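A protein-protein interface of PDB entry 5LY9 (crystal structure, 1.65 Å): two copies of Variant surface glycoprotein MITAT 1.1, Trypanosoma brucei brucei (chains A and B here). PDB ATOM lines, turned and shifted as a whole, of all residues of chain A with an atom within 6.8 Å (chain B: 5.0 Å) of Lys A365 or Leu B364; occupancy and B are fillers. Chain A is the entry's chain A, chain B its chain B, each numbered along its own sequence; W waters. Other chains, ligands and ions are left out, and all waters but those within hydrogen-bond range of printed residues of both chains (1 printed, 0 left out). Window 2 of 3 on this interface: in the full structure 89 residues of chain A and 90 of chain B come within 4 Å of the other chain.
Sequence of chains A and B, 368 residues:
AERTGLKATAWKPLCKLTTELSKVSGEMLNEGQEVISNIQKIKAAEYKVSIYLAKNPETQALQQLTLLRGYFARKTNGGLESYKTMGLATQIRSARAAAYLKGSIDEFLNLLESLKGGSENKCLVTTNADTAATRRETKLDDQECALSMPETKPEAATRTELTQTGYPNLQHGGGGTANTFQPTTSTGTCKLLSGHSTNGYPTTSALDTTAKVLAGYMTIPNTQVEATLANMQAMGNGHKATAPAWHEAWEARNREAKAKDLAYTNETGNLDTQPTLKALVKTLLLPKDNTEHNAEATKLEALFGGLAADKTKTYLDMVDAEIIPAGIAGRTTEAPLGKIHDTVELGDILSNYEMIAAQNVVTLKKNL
Val B361 touches Asn A360.
Lys A365 touches Glu B58 (CD to OE2, 3.1 Å).
Lys A365 touches Leu B364 (NZ to CD2, 3.7 Å).
Lys A365 touches just these residues of chain B: Glu B58 and Leu B364.
Leu B364 touches just one residue of chain A: Lys A365 (3.7 Å).
Of the printed residues of chain A, Glu B58 touches Lys A365 (3.1 Å).
Of the printed residues of chain B, Asn A360 touches Val B361 (3.8 Å).
Of the printed residues of chain A, Val B361 touches Asn A360 (3.8 Å).
The nearest printed residue of chain B that does not touch Lys A365 is Asn B360 (5.1 Å).
The nearest printed residue of chain A that does not touch Glu B58 is Val A362 (4.1 Å).
Printed residues of chain A that touch a printed residue of chain B: Asn A360 and Lys A365.
Among the printed residues, 3 pairs touch across the chains.
Among the printed residues, no Asp or Glu carboxylate lies within 4 Å of a Lys or Arg side-chain nitrogen of the other chain.
Asn A360 touches Val B361, but with the chains exchanged Val A361 does not touch Asn B360 (4.1 Å).
Lys A365 touches Leu B364, but with the chains exchanged Leu A364 does not touch Lys B365 (4.02 Å).
Of the 3 pairs that touch across the chains among the printed residues, none has its exchanged pair printed and touching as well.
Water W1 bridges OD1 of Asn B360 and NZ of Lys A365.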
ATOM      1  N   ASN A 360     -24.017  13.150 -13.040  1.00  0.00           N
ATOM      2  CA  ASN A 360     -23.719  12.491 -14.325  1.00  0.00           C
ATOM      3  C   ASN A 360     -22.937  11.204 -14.120  1.00  0.00           C
ATOM      4  O   ASN A 360     -23.241  10.188 -14.727  1.00  0.00           O
ATOM      5  CB  ASN A 360     -22.880  13.444 -15.247  1.00  0.00           C
ATOM      6  CG  ASN A 360     -22.632  12.865 -16.649  1.00  0.00           C
ATOM      7  OD1 ASN A 360     -23.553  12.267 -17.230  1.00  0.00           O
ATOM      8  ND2 ASN A 360     -21.393  13.037 -17.219  1.00  0.00           N
ATOM      9  N   VAL A 361     -21.896  11.273 -13.290  1.00  0.00           N
ATOM     10  CA  VAL A 361     -21.072  10.125 -12.972  1.00  0.00           C
ATOM     11  C   VAL A 361     -21.866   9.040 -12.281  1.00  0.00           C
ATOM     12  O   VAL A 361     -21.800   7.895 -12.657  1.00  0.00           O
ATOM     13  CB  VAL A 361     -19.859  10.497 -12.135  1.00  0.00           C
ATOM     14  CG1 VAL A 361     -19.112   9.251 -11.653  1.00  0.00           C
ATOM     15  CG2 VAL A 361     -18.956  11.404 -12.929  1.00  0.00           C
ATOM     16  N   VAL A 362     -22.674   9.406 -11.319  1.00  0.00           N
ATOM     17  CA  VAL A 362     -23.456   8.481 -10.573  1.00  0.00           C
ATOM     18  C   VAL A 362     -24.395   7.735 -11.550  1.00  0.00           C
ATOM     19  O   VAL A 362     -24.540   6.492 -11.432  1.00  0.00           O
ATOM     20  CB  VAL A 362     -24.303   9.206  -9.548  1.00  0.00           C
ATOM     21  CG1 VAL A 362     -25.356   8.298  -8.961  1.00  0.00           C
ATOM     22  CG2 VAL A 362     -23.461   9.806  -8.420  1.00  0.00           C
ATOM     23  N   THR A 363     -25.038   8.479 -12.459  1.00  0.00           N
ATOM     24  CA  THR A 363     -25.987   7.915 -13.441  1.00  0.00           C
ATOM     25  C   THR A 363     -25.228   6.964 -14.372  1.00  0.00           C
ATOM     26  O   THR A 363     -25.684   5.823 -14.622  1.00  0.00           O
ATOM     27  CB  THR A 363     -26.629   9.030 -14.275  1.00  0.00           C
ATOM     28  OG1 THR A 363     -27.406   9.874 -13.427  1.00  0.00           O
ATOM     29  CG2 THR A 363     -27.532   8.473 -15.449  1.00  0.00           C
ATOM     30  N   LEU A 364     -24.079   7.417 -14.880  1.00  0.00           N
ATOM     31  CA  LEU A 364     -23.298   6.587 -15.757  1.00  0.00           C
ATOM     32  C   LEU A 364     -23.003   5.283 -15.030  1.00  0.00           C
ATOM     33  O   LEU A 364     -23.392   4.213 -15.509  1.00  0.00           O
ATOM     34  CB  LEU A 364     -22.016   7.261 -16.258  1.00  0.00           C
ATOM     35  CG  LEU A 364     -22.274   8.339 -17.296  1.00  0.00           C
ATOM     36  CD1 LEU A 364     -21.068   9.218 -17.569  1.00  0.00           C
ATOM     37  CD2 LEU A 364     -22.800   7.742 -18.601  1.00  0.00           C
ATOM     38  N   LYS A 365     -22.387   5.372 -13.860  1.00  0.00           N
ATOM     39  CA  LYS A 365     -21.980   4.194 -13.123  1.00  0.00           C
ATOM     40  C   LYS A 365     -23.126   3.262 -12.856  1.00  0.00           C
ATOM     41  O   LYS A 365     -22.940   2.042 -12.893  1.00  0.00           O
ATOM     42  CB  LYS A 365     -21.259   4.567 -11.824  1.00  0.00           C
ATOM     43  CG  LYS A 365     -19.911   5.171 -12.122  1.00  0.00           C
ATOM     44  CD  LYS A 365     -19.000   5.160 -10.924  1.00  0.00           C
ATOM     45  CE  LYS A 365     -17.559   5.164 -11.360  1.00  0.00           C
ATOM     46  NZ  LYS A 365     -17.093   3.792 -11.747  1.00  0.00           N
ATOM     47  N   LYS A 366     -24.298   3.836 -12.612  1.00  0.00           N
ATOM     48  CA  LYS A 366     -25.530   3.088 -12.481  1.00  0.00           C
ATOM     49  C   LYS A 366     -25.914   2.304 -13.762  1.00  0.00           C
ATOM     50  O   LYS A 366     -26.404   1.170 -13.670  1.00  0.00           O
ATOM     51  CB  LYS A 366     -26.652   4.043 -12.084  1.00  0.00           C
ATOM     52  CG  LYS A 366     -28.038   3.437 -11.924  1.00  0.00           C
ATOM     53  CD  LYS A 366     -29.089   4.520 -11.694  1.00  0.00           C
ATOM     54  CE  LYS A 366     -28.869   5.316 -10.394  1.00  0.00           C
ATOM     55  NZ  LYS A 366     -28.251   6.685 -10.566  1.00  0.00           N
ATOM     56  N   ASN A 367     -25.732   2.920 -14.930  1.00  0.00           N
ATOM     57  CA  ASN A 367     -26.066   2.285 -16.210  1.00  0.00           C
ATOM     58  C   ASN A 367     -25.074   1.168 -16.518  1.00  0.00           C
ATOM     59  O   ASN A 367     -25.453   0.164 -17.118  1.00  0.00           O
ATOM     60  CB  ASN A 367     -26.094   3.296 -17.369  1.00  0.00           C
ATOM     61  CG  ASN A 367     -27.155   4.363 -17.193  1.00  0.00           C
ATOM     62  OD1 ASN A 367     -28.066   4.250 -16.360  1.00  0.00           O
ATOM     63  ND2 ASN A 367     -27.025   5.432 -17.972  1.00  0.00           N
ATOM     64  N   LEU A 368     -23.820   1.399 -16.126  1.00  0.00           N
ATOM     65  CA  LEU A 368     -22.746   0.398 -15.953  1.00  0.00           C
ATOM     66  C   LEU A 368     -21.663   0.644 -16.993  1.00  0.00           C
ATOM     67  O   LEU A 368     -20.568   1.092 -16.654  1.00  0.00           O
ATOM     68  CB  LEU A 368     -23.196  -1.084 -15.947  1.00  0.00           C
ATOM     69  CG  LEU A 368     -24.210  -1.629 -14.901  1.00  0.00           C
ATOM     70  CD1 LEU A 368     -24.477  -3.115 -15.150  1.00  0.00           C
ATOM     71  CD2 LEU A 368     -23.794  -1.392 -13.449  1.00  0.00           C
ATOM     72  N   GLU B  58     -19.262  10.354  -6.410  1.00  0.00           N
ATOM     73  CA  GLU B  58     -20.304   9.473  -5.883  1.00  0.00           C
ATOM     74  C   GLU B  58     -20.629   9.683  -4.438  1.00  0.00           C
ATOM     75  O   GLU B  58     -21.434   8.950  -3.833  1.00  0.00           O
ATOM     76  CB  GLU B  58     -19.944   8.027  -6.163  1.00  0.00           C
ATOM     77  CG  GLU B  58     -19.672   7.835  -7.620  1.00  0.00           C
ATOM     78  CD  GLU B  58     -19.383   6.394  -7.906  1.00  0.00           C
ATOM     79  OE1 GLU B  58     -20.381   5.630  -7.913  1.00  0.00           O
ATOM     80  OE2 GLU B  58     -18.182   6.085  -8.063  1.00  0.00           O
ATOM     81  N   ASN B 360     -12.214  10.843 -16.512  1.00  0.00           N
ATOM     82  CA  ASN B 360     -13.077   9.748 -15.915  1.00  0.00           C
ATOM     83  C   ASN B 360     -14.380   9.559 -16.658  1.00  0.00           C
ATOM     84  O   ASN B 360     -14.786   8.410 -16.966  1.00  0.00           O
ATOM     85  CB  ASN B 360     -13.375  10.056 -14.437  1.00  0.00           C
ATOM     86  CG  ASN B 360     -14.229   8.980 -13.727  1.00  0.00           C
ATOM     87  OD1 ASN B 360     -13.892   7.787 -13.717  1.00  0.00           O
ATOM     88  ND2 ASN B 360     -15.315   9.423 -13.071  1.00  0.00           N
ATOM     89  N   VAL B 361     -15.046  10.661 -16.970  1.00  0.00           N
ATOM     90  CA  VAL B 361     -16.277  10.613 -17.678  1.00  0.00           C
ATOM     91  C   VAL B 361     -16.053  10.016 -19.087  1.00  0.00           C
ATOM     92  O   VAL B 361     -16.802   9.149 -19.513  1.00  0.00           O
ATOM     93  CB  VAL B 361     -16.935  11.982 -17.829  1.00  0.00           C
ATOM     94  CG1 VAL B 361     -18.160  11.887 -18.745  1.00  0.00           C
ATOM     95  CG2 VAL B 361     -17.344  12.558 -16.498  1.00  0.00           C
ATOM     96  N   VAL B 362     -15.058  10.535 -19.801  1.00  0.00           N
ATOM     97  CA  VAL B 362     -14.721  10.081 -21.127  1.00  0.00           C
ATOM     98  C   VAL B 362     -14.421   8.552 -21.070  1.00  0.00           C
ATOM     99  O   VAL B 362     -14.937   7.783 -21.908  1.00  0.00           O
ATOM    100  CB  VAL B 362     -13.541  10.887 -21.697  1.00  0.00           C
ATOM    101  CG1 VAL B 362     -13.011  10.280 -22.994  1.00  0.00           C
ATOM    102  CG2 VAL B 362     -13.950  12.322 -21.953  1.00  0.00           C
ATOM    103  N   THR B 363     -13.664   8.099 -20.075  1.00  0.00           N
ATOM    104  CA  THR B 363     -13.458   6.652 -19.879  1.00  0.00           C
ATOM    105  C   THR B 363     -14.744   5.838 -19.600  1.00  0.00           C
ATOM    106  O   THR B 363     -14.952   4.752 -20.203  1.00  0.00           O
ATOM    107  CB  THR B 363     -12.453   6.431 -18.773  1.00  0.00           C
ATOM    108  OG1 THR B 363     -11.257   7.127 -19.127  1.00  0.00           O
ATOM    109  CG2 THR B 363     -12.111   4.927 -18.623  1.00  0.00           C
ATOM    110  N   LEU B 364     -15.590   6.321 -18.701  1.00  0.00           N
ATOM    111  CA  LEU B 364     -16.852   5.629 -18.378  1.00  0.00           C
ATOM    112  C   LEU B 364     -17.735   5.537 -19.618  1.00  0.00           C
ATOM    113  O   LEU B 364     -18.360   4.491 -19.867  1.00  0.00           O
ATOM    114  CB  LEU B 364     -17.656   6.347 -17.302  1.00  0.00           C
ATOM    115  CG  LEU B 364     -17.176   6.266 -15.864  1.00  0.00           C
ATOM    116  CD1 LEU B 364     -17.987   7.234 -15.005  1.00  0.00           C
ATOM    117  CD2 LEU B 364     -17.307   4.887 -15.283  1.00  0.00           C
ATOM    118  N   LYS B 365     -17.808   6.623 -20.381  1.00  0.00           N
ATOM    119  CA  LYS B 365     -18.626   6.623 -21.578  1.00  0.00           C
ATOM    120  C   LYS B 365     -18.041   5.712 -22.660  1.00  0.00           C
ATOM    121  O   LYS B 365     -18.784   5.069 -23.397  1.00  0.00           O
ATOM    122  CB  LYS B 365     -18.912   8.038 -22.092  1.00  0.00           C
ATOM    123  CG  LYS B 365     -20.231   8.598 -21.578  1.00  0.00           C
ATOM    124  CD  LYS B 365     -20.929   9.452 -22.621  1.00  0.00           C
ATOM    125  CE  LYS B 365     -21.595   8.624 -23.726  1.00  0.00           C
ATOM    126  NZ  LYS B 365     -22.684   7.694 -23.272  1.00  0.00           N
ATOM    127  N   LYS B 366     -16.722   5.617 -22.725  1.00  0.00           N
ATOM    128  CA  LYS B 366     -16.077   4.706 -23.645  1.00  0.00           C
ATOM    129  C   LYS B 366     -16.396   3.257 -23.290  1.00  0.00           C
ATOM    130  O   LYS B 366     -16.737   2.450 -24.175  1.00  0.00           O
ATOM    131  CB  LYS B 366     -14.573   4.925 -23.628  1.00  0.00           C
ATOM    132  CG  LYS B 366     -13.781   3.977 -24.504  1.00  0.00           C
ATOM    133  CD  LYS B 366     -12.317   4.386 -24.552  1.00  0.00           C
ATOM    134  CE  LYS B 366     -11.603   4.314 -23.199  1.00  0.00           C
ATOM    135  NZ  LYS B 366     -11.639   2.971 -22.540  1.00  0.00           N
ATOM    136  N   ASN B 367     -16.274   2.937 -22.003  1.00  0.00           N
ATOM    137  CA  ASN B 367     -16.516   1.572 -21.513  1.00  0.00           C
ATOM    138  C   ASN B 367     -18.005   1.196 -21.536  1.00  0.00           C
ATOM    139  O   ASN B 367     -18.889   2.062 -21.586  1.00  0.00           O
ATOM    140  CB  ASN B 367     -15.962   1.406 -20.092  1.00  0.00           C
ATOM    141  CG  ASN B 367     -14.462   1.671 -20.004  1.00  0.00           C
ATOM    142  OD1 ASN B 367     -13.807   2.024 -20.996  1.00  0.00           O
ATOM    143  ND2 ASN B 367     -13.915   1.527 -18.799  1.00  0.00           N
HETATM  144  O   HOH W   1     -14.657   5.996 -12.173  1.00  0.00           O
